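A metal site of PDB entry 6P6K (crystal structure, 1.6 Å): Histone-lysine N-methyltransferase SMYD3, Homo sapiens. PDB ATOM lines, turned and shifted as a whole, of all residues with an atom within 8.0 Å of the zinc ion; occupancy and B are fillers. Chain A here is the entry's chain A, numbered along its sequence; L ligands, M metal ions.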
ATOM      1  N   HIS A 210     -30.818 -21.207 -22.557  1.00  0.00           N
ATOM      2  CA  HIS A 210     -30.063 -22.028 -21.638  1.00  0.00           C
ATOM      3  C   HIS A 210     -30.454 -21.760 -20.195  1.00  0.00           C
ATOM      4  O   HIS A 210     -30.698 -20.611 -19.811  1.00  0.00           O
ATOM      5  CB  HIS A 210     -28.574 -21.758 -21.796  1.00  0.00           C
ATOM      6  CG  HIS A 210     -27.755 -22.275 -20.658  1.00  0.00           C
ATOM      7  ND1 HIS A 210     -27.289 -23.570 -20.601  1.00  0.00           N
ATOM      8  CD2 HIS A 210     -27.363 -21.672 -19.505  1.00  0.00           C
ATOM      9  CE1 HIS A 210     -26.628 -23.744 -19.471  1.00  0.00           C
ATOM     10  NE2 HIS A 210     -26.661 -22.609 -18.789  1.00  0.00           N
ATOM     11  N   SER A 211     -30.451 -22.812 -19.379  1.00  0.00           N
ATOM     12  CA  SER A 211     -30.439 -22.673 -17.934  1.00  0.00           C
ATOM     13  C   SER A 211     -29.528 -23.746 -17.345  1.00  0.00           C
ATOM     14  O   SER A 211     -29.486 -24.870 -17.843  1.00  0.00           O
ATOM     15  CB  SER A 211     -31.837 -22.823 -17.325  1.00  0.00           C
ATOM     16  OG  SER A 211     -31.754 -22.836 -15.908  1.00  0.00           O
ATOM     17  N   CYS A 212     -28.794 -23.372 -16.295  1.00  0.00           N
ATOM     18  CA  CYS A 212     -28.017 -24.328 -15.523  1.00  0.00           C
ATOM     19  C   CYS A 212     -28.885 -25.181 -14.606  1.00  0.00           C
ATOM     20  O   CYS A 212     -28.357 -26.090 -13.944  1.00  0.00           O
ATOM     21  CB  CYS A 212     -26.958 -23.618 -14.677  1.00  0.00           C
ATOM     22  SG  CYS A 212     -25.901 -22.510 -15.649  1.00  0.00           S
ATOM     23  N   ASP A 213     -30.183 -24.902 -14.526  1.00  0.00           N
ATOM     24  CA  ASP A 213     -31.138 -25.741 -13.816  1.00  0.00           C
ATOM     25  C   ASP A 213     -32.438 -25.741 -14.625  1.00  0.00           C
ATOM     26  O   ASP A 213     -33.417 -25.064 -14.294  1.00  0.00           O
ATOM     27  CB  ASP A 213     -31.337 -25.229 -12.384  1.00  0.00           C
ATOM     28  CG  ASP A 213     -32.361 -26.004 -11.617  1.00  0.00           C
ATOM     29  OD1 ASP A 213     -32.656 -27.166 -11.979  1.00  0.00           O
ATOM     30  OD2 ASP A 213     -32.883 -25.423 -10.661  1.00  0.00           O
ATOM     31  N   CYS A 242     -30.321 -27.184 -20.608  1.00  0.00           N
ATOM     32  CA  CYS A 242     -28.946 -26.895 -20.233  1.00  0.00           C
ATOM     33  C   CYS A 242     -28.048 -27.203 -21.433  1.00  0.00           C
ATOM     34  O   CYS A 242     -27.973 -28.351 -21.879  1.00  0.00           O
ATOM     35  CB  CYS A 242     -28.535 -27.713 -19.007  1.00  0.00           C
ATOM     36  SG  CYS A 242     -26.885 -27.244 -18.446  1.00  0.00           S
ATOM     37  N   LEU A 244     -24.942 -27.387 -21.543  1.00  0.00           N
ATOM     38  CA  LEU A 244     -23.624 -27.844 -21.114  1.00  0.00           C
ATOM     39  C   LEU A 244     -23.712 -29.131 -20.299  1.00  0.00           C
ATOM     40  O   LEU A 244     -24.719 -29.427 -19.657  1.00  0.00           O
ATOM     41  CB  LEU A 244     -22.952 -26.810 -20.218  1.00  0.00           C
ATOM     42  CG  LEU A 244     -22.913 -25.417 -20.819  1.00  0.00           C
ATOM     43  CD1 LEU A 244     -22.290 -24.459 -19.800  1.00  0.00           C
ATOM     44  CD2 LEU A 244     -22.103 -25.469 -22.084  1.00  0.00           C
ATOM     45  N   SER A 250     -19.116 -23.368 -12.006  1.00  0.00           N
ATOM     46  CA  SER A 250     -19.683 -22.127 -12.545  1.00  0.00           C
ATOM     47  C   SER A 250     -18.642 -21.330 -13.329  1.00  0.00           C
ATOM     48  O   SER A 250     -18.986 -20.641 -14.290  1.00  0.00           O
ATOM     49  CB  SER A 250     -20.273 -21.277 -11.418  1.00  0.00           C
ATOM     50  OG  SER A 250     -19.275 -20.896 -10.481  1.00  0.00           O
ATOM     51  N   ARG A 253     -18.575 -23.052 -16.658  1.00  0.00           N
ATOM     52  CA  ARG A 253     -19.769 -22.699 -17.405  1.00  0.00           C
ATOM     53  C   ARG A 253     -19.674 -21.267 -17.907  1.00  0.00           C
ATOM     54  O   ARG A 253     -20.014 -20.982 -19.061  1.00  0.00           O
ATOM     55  CB  ARG A 253     -21.025 -22.892 -16.561  1.00  0.00           C
ATOM     56  CG  ARG A 253     -21.243 -24.338 -16.153  1.00  0.00           C
ATOM     57  CD  ARG A 253     -22.680 -24.576 -15.732  1.00  0.00           C
ATOM     58  NE  ARG A 253     -23.118 -23.690 -14.658  1.00  0.00           N
ATOM     59  CZ  ARG A 253     -22.850 -23.867 -13.363  1.00  0.00           C
ATOM     60  NH1 ARG A 253     -22.112 -24.891 -12.963  1.00  0.00           N
ATOM     61  NH2 ARG A 253     -23.311 -23.011 -12.468  1.00  0.00           N
ATOM     62  N   ARG A 254     -19.182 -20.353 -17.067  1.00  0.00           N
ATOM     63  CA  ARG A 254     -19.022 -18.970 -17.487  1.00  0.00           C
ATOM     64  C   ARG A 254     -18.142 -18.872 -18.723  1.00  0.00           C
ATOM     65  O   ARG A 254     -18.452 -18.123 -19.666  1.00  0.00           O
ATOM     66  CB  ARG A 254     -18.422 -18.142 -16.352  1.00  0.00           C
ATOM     67  CG  ARG A 254     -18.071 -16.713 -16.766  1.00  0.00           C
ATOM     68  CD  ARG A 254     -17.637 -15.849 -15.576  1.00  0.00           C
ATOM     69  NE  ARG A 254     -18.767 -15.658 -14.667  1.00  0.00           N
ATOM     70  CZ  ARG A 254     -18.851 -16.227 -13.467  1.00  0.00           C
ATOM     71  NH1 ARG A 254     -17.852 -16.973 -13.007  1.00  0.00           N
ATOM     72  NH2 ARG A 254     -19.930 -16.009 -12.712  1.00  0.00           N
ATOM     73  N   LEU A 257     -20.062 -20.382 -21.796  1.00  0.00           N
ATOM     74  CA  LEU A 257     -21.220 -19.595 -22.188  1.00  0.00           C
ATOM     75  C   LEU A 257     -20.800 -18.262 -22.789  1.00  0.00           C
ATOM     76  O   LEU A 257     -21.453 -17.761 -23.698  1.00  0.00           O
ATOM     77  CB  LEU A 257     -22.165 -19.410 -20.998  1.00  0.00           C
ATOM     78  CG  LEU A 257     -22.836 -20.691 -20.475  1.00  0.00           C
ATOM     79  CD1 LEU A 257     -23.740 -20.344 -19.313  1.00  0.00           C
ATOM     80  CD2 LEU A 257     -23.600 -21.408 -21.585  1.00  0.00           C
ATOM     81  N   PHE A 263     -23.023 -14.988 -23.750  1.00  0.00           N
ATOM     82  CA  PHE A 263     -23.849 -14.412 -22.688  1.00  0.00           C
ATOM     83  C   PHE A 263     -23.287 -14.725 -21.309  1.00  0.00           C
ATOM     84  O   PHE A 263     -22.456 -15.623 -21.142  1.00  0.00           O
ATOM     85  CB  PHE A 263     -25.326 -14.812 -22.782  1.00  0.00           C
ATOM     86  CG  PHE A 263     -25.618 -16.238 -22.407  1.00  0.00           C
ATOM     87  CD1 PHE A 263     -25.591 -17.232 -23.371  1.00  0.00           C
ATOM     88  CD2 PHE A 263     -25.954 -16.565 -21.111  1.00  0.00           C
ATOM     89  CE1 PHE A 263     -25.878 -18.534 -23.041  1.00  0.00           C
ATOM     90  CE2 PHE A 263     -26.236 -17.893 -20.763  1.00  0.00           C
ATOM     91  CZ  PHE A 263     -26.195 -18.860 -21.737  1.00  0.00           C
ATOM     92  N   GLU A 264     -23.744 -13.925 -20.343  1.00  0.00           N
ATOM     93  CA  GLU A 264     -23.408 -14.043 -18.929  1.00  0.00           C
ATOM     94  C   GLU A 264     -24.613 -14.639 -18.234  1.00  0.00           C
ATOM     95  O   GLU A 264     -25.732 -14.147 -18.387  1.00  0.00           O
ATOM     96  CB  GLU A 264     -23.085 -12.665 -18.335  1.00  0.00           C
ATOM     97  CG  GLU A 264     -22.264 -11.724 -19.250  1.00  0.00           C
ATOM     98  CD  GLU A 264     -20.858 -12.231 -19.471  1.00  0.00           C
ATOM     99  OE1 GLU A 264     -20.176 -11.683 -20.339  1.00  0.00           O
ATOM    100  OE2 GLU A 264     -20.459 -13.180 -18.755  1.00  0.00           O
ATOM    101  N   CYS A 265     -24.411 -15.714 -17.480  1.00  0.00           N
ATOM    102  CA  CYS A 265     -25.571 -16.395 -16.913  1.00  0.00           C
ATOM    103  C   CYS A 265     -25.878 -15.855 -15.532  1.00  0.00           C
ATOM    104  O   CYS A 265     -25.005 -15.804 -14.666  1.00  0.00           O
ATOM    105  CB  CYS A 265     -25.358 -17.895 -16.858  1.00  0.00           C
ATOM    106  SG  CYS A 265     -26.839 -18.652 -16.089  1.00  0.00           S
ATOM    107  N   ASP A 266     -27.148 -15.468 -15.343  1.00  0.00           N
ATOM    108  CA  ASP A 266     -27.613 -14.806 -14.138  1.00  0.00           C
ATOM    109  C   ASP A 266     -28.307 -15.753 -13.165  1.00  0.00           C
ATOM    110  O   ASP A 266     -28.796 -15.295 -12.124  1.00  0.00           O
ATOM    111  CB  ASP A 266     -28.572 -13.649 -14.512  1.00  0.00           C
ATOM    112  CG  ASP A 266     -29.746 -14.103 -15.385  1.00  0.00           C
ATOM    113  OD1 ASP A 266     -29.734 -15.237 -15.915  1.00  0.00           O
ATOM    114  OD2 ASP A 266     -30.712 -13.309 -15.537  1.00  0.00           O
ATOM    115  N   CYS A 267     -28.333 -17.058 -13.463  1.00  0.00           N
ATOM    116  CA  CYS A 267     -29.160 -17.993 -12.716  1.00  0.00           C
ATOM    117  C   CYS A 267     -28.674 -18.135 -11.272  1.00  0.00           C
ATOM    118  O   CYS A 267     -27.572 -17.728 -10.899  1.00  0.00           O
ATOM    119  CB  CYS A 267     -29.190 -19.353 -13.416  1.00  0.00           C
ATOM    120  SG  CYS A 267     -27.787 -20.447 -13.047  1.00  0.00           S
ATOM    121  N   PHE A 268     -29.552 -18.682 -10.428  1.00  0.00           N
ATOM    122  CA  PHE A 268     -29.213 -18.849  -9.020  1.00  0.00           C
ATOM    123  C   PHE A 268     -27.939 -19.679  -8.850  1.00  0.00           C
ATOM    124  O   PHE A 268     -27.118 -19.378  -7.979  1.00  0.00           O
ATOM    125  CB  PHE A 268     -30.370 -19.533  -8.279  1.00  0.00           C
ATOM    126  CG  PHE A 268     -29.968 -20.124  -6.967  1.00  0.00           C
ATOM    127  CD1 PHE A 268     -29.898 -19.324  -5.834  1.00  0.00           C
ATOM    128  CD2 PHE A 268     -29.663 -21.477  -6.859  1.00  0.00           C
ATOM    129  CE1 PHE A 268     -29.537 -19.861  -4.610  1.00  0.00           C
ATOM    130  CE2 PHE A 268     -29.284 -22.013  -5.626  1.00  0.00           C
ATOM    131  CZ  PHE A 268     -29.225 -21.201  -4.518  1.00  0.00           C
ATOM    132  N   ARG A 269     -27.778 -20.723  -9.665  1.00  0.00           N
ATOM    133  CA  ARG A 269     -26.604 -21.568  -9.516  1.00  0.00           C
ATOM    134  C   ARG A 269     -25.328 -20.786  -9.795  1.00  0.00           C
ATOM    135  O   ARG A 269     -24.334 -20.945  -9.075  1.00  0.00           O
ATOM    136  CB  ARG A 269     -26.698 -22.790 -10.436  1.00  0.00           C
ATOM    137  CG  ARG A 269     -27.792 -23.773 -10.061  1.00  0.00           C
ATOM    138  CD  ARG A 269     -27.551 -25.102 -10.736  1.00  0.00           C
ATOM    139  NE  ARG A 269     -26.312 -25.669 -10.240  1.00  0.00           N
ATOM    140  CZ  ARG A 269     -25.425 -26.310 -11.003  1.00  0.00           C
ATOM    141  NH1 ARG A 269     -25.658 -26.473 -12.307  1.00  0.00           N
ATOM    142  NH2 ARG A 269     -24.303 -26.756 -10.467  1.00  0.00           N
ATOM    143  N   CYS A 270     -25.356 -19.915 -10.800  1.00  0.00           N
ATOM    144  CA  CYS A 270     -24.139 -19.175 -11.116  1.00  0.00           C
ATOM    145  C   CYS A 270     -23.897 -18.069 -10.101  1.00  0.00           C
ATOM    146  O   CYS A 270     -22.759 -17.857  -9.672  1.00  0.00           O
ATOM    147  CB  CYS A 270     -24.232 -18.629 -12.540  1.00  0.00           C
ATOM    148  SG  CYS A 270     -24.172 -19.946 -13.771  1.00  0.00           S
ATOM    149  N   GLN A 271     -24.965 -17.441  -9.632  1.00  0.00           N
ATOM    150  CA  GLN A 271     -24.789 -16.412  -8.612  1.00  0.00           C
ATOM    151  C   GLN A 271     -24.256 -16.984  -7.305  1.00  0.00           C
ATOM    152  O   GLN A 271     -23.546 -16.282  -6.581  1.00  0.00           O
ATOM    153  CB  GLN A 271     -26.106 -15.658  -8.386  1.00  0.00           C
ATOM    154  CG  GLN A 271     -25.917 -14.433  -7.538  1.00  0.00           C
ATOM    155  CD  GLN A 271     -26.922 -13.337  -7.823  1.00  0.00           C
ATOM    156  OE1 GLN A 271     -27.739 -13.447  -8.742  1.00  0.00           O
ATOM    157  NE2 GLN A 271     -26.853 -12.273  -7.044  1.00  0.00           N
HETATM  158  N1  LIG L   1     -32.227 -16.543 -27.853  1.00  0.00           N
HETATM  159  C1  LIG L   1     -31.836 -17.333 -29.003  1.00  0.00           C
HETATM  160  C2  LIG L   1     -32.384 -16.675 -30.280  1.00  0.00           C
HETATM  161  O1  LIG L   1     -32.330 -17.257 -31.363  1.00  0.00           O
HETATM  162  O2  LIG L   1     -32.874 -15.542 -30.216  1.00  0.00           O
HETATM  163  C3  LIG L   1     -32.312 -18.773 -28.834  1.00  0.00           C
HETATM  164  C4  LIG L   1     -31.254 -19.654 -28.170  1.00  0.00           C
HETATM  165  S1  LIG L   1     -29.801 -19.857 -29.254  1.00  0.00           S
HETATM  166  C5  LIG L   1     -29.583 -21.647 -29.298  1.00  0.00           C
HETATM  167  C6  LIG L   1     -28.398 -19.465 -28.173  1.00  0.00           C
HETATM  168  C7  LIG L   1     -28.276 -17.968 -27.909  1.00  0.00           C
HETATM  169  O3  LIG L   1     -29.350 -17.521 -27.102  1.00  0.00           O
HETATM  170  C8  LIG L   1     -27.037 -17.620 -27.108  1.00  0.00           C
HETATM  171  O4  LIG L   1     -25.905 -17.553 -27.932  1.00  0.00           O
HETATM  172  C9  LIG L   1     -27.414 -16.306 -26.445  1.00  0.00           C
HETATM  173  O5  LIG L   1     -27.347 -15.281 -27.425  1.00  0.00           O
HETATM  174  C10 LIG L   1     -28.879 -16.563 -26.161  1.00  0.00           C
HETATM  175  N2  LIG L   1     -29.102 -17.156 -24.833  1.00  0.00           N
HETATM  176  C11 LIG L   1     -29.362 -18.482 -24.564  1.00  0.00           C
HETATM  177  N3  LIG L   1     -29.543 -18.649 -23.233  1.00  0.00           N
HETATM  178  C12 LIG L   1     -29.413 -17.440 -22.636  1.00  0.00           C
HETATM  179  C13 LIG L   1     -29.497 -17.038 -21.313  1.00  0.00           C
HETATM  180  N4  LIG L   1     -29.748 -17.885 -20.318  1.00  0.00           N
HETATM  181  N5  LIG L   1     -29.295 -15.713 -21.025  1.00  0.00           N
HETATM  182  C14 LIG L   1     -29.035 -14.812 -22.021  1.00  0.00           C
HETATM  183  N6  LIG L   1     -28.944 -15.209 -23.333  1.00  0.00           N
HETATM  184  C15 LIG L   1     -29.140 -16.498 -23.639  1.00  0.00           C
HETATM  185 ZN    ZN M   1     -26.260 -20.289 -14.669  1.00  0.00          ZN
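Within 4 Å of the zinc ion: Cys 212, Cys 265, Cys 267 and Cys 270.
The nearest printed residue that does not touch the zinc ion is Arg 253 (4.6 Å).
O of His 210 lies within hydrogen-bond range of N4 of the ligand, at 2.9 Å.
A nitrogen (N3) of the ligand is in hydrogen-bond range of the backbone NH of His 210, 2.9 Å away.
The zinc ion is bound by the side-chain sulfur (SG) of Cys 267 (2.2 Å), the side-chain sulfur (SG) of Cys 265 (2.2 Å), the side-chain sulfur (SG) of Cys 270 (2.3 Å) and the side-chain sulfur (SG) of Cys 212 (2.5 Å).
The zinc ion has four donor atoms within binding distance.
N of Cys 212 lies within hydrogen-bond range of NE2 of His 210, 3.4 Å away.
The side-chain sulfur (SG) of Cys 267 sits close to the backbone NH (N) of Arg 269.
The guanidinium group of Arg 269 lies within hydrogen-bond range of the backbone carbonyl oxygen of Cys 212, at 3.2 Å.
The guanidinium group (NH2) of Arg 253 lies close to the side-chain sulfur (SG) of Cys 270.
SG of Cys 212 sits close to NE of Arg 253, 3.2 Å away.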
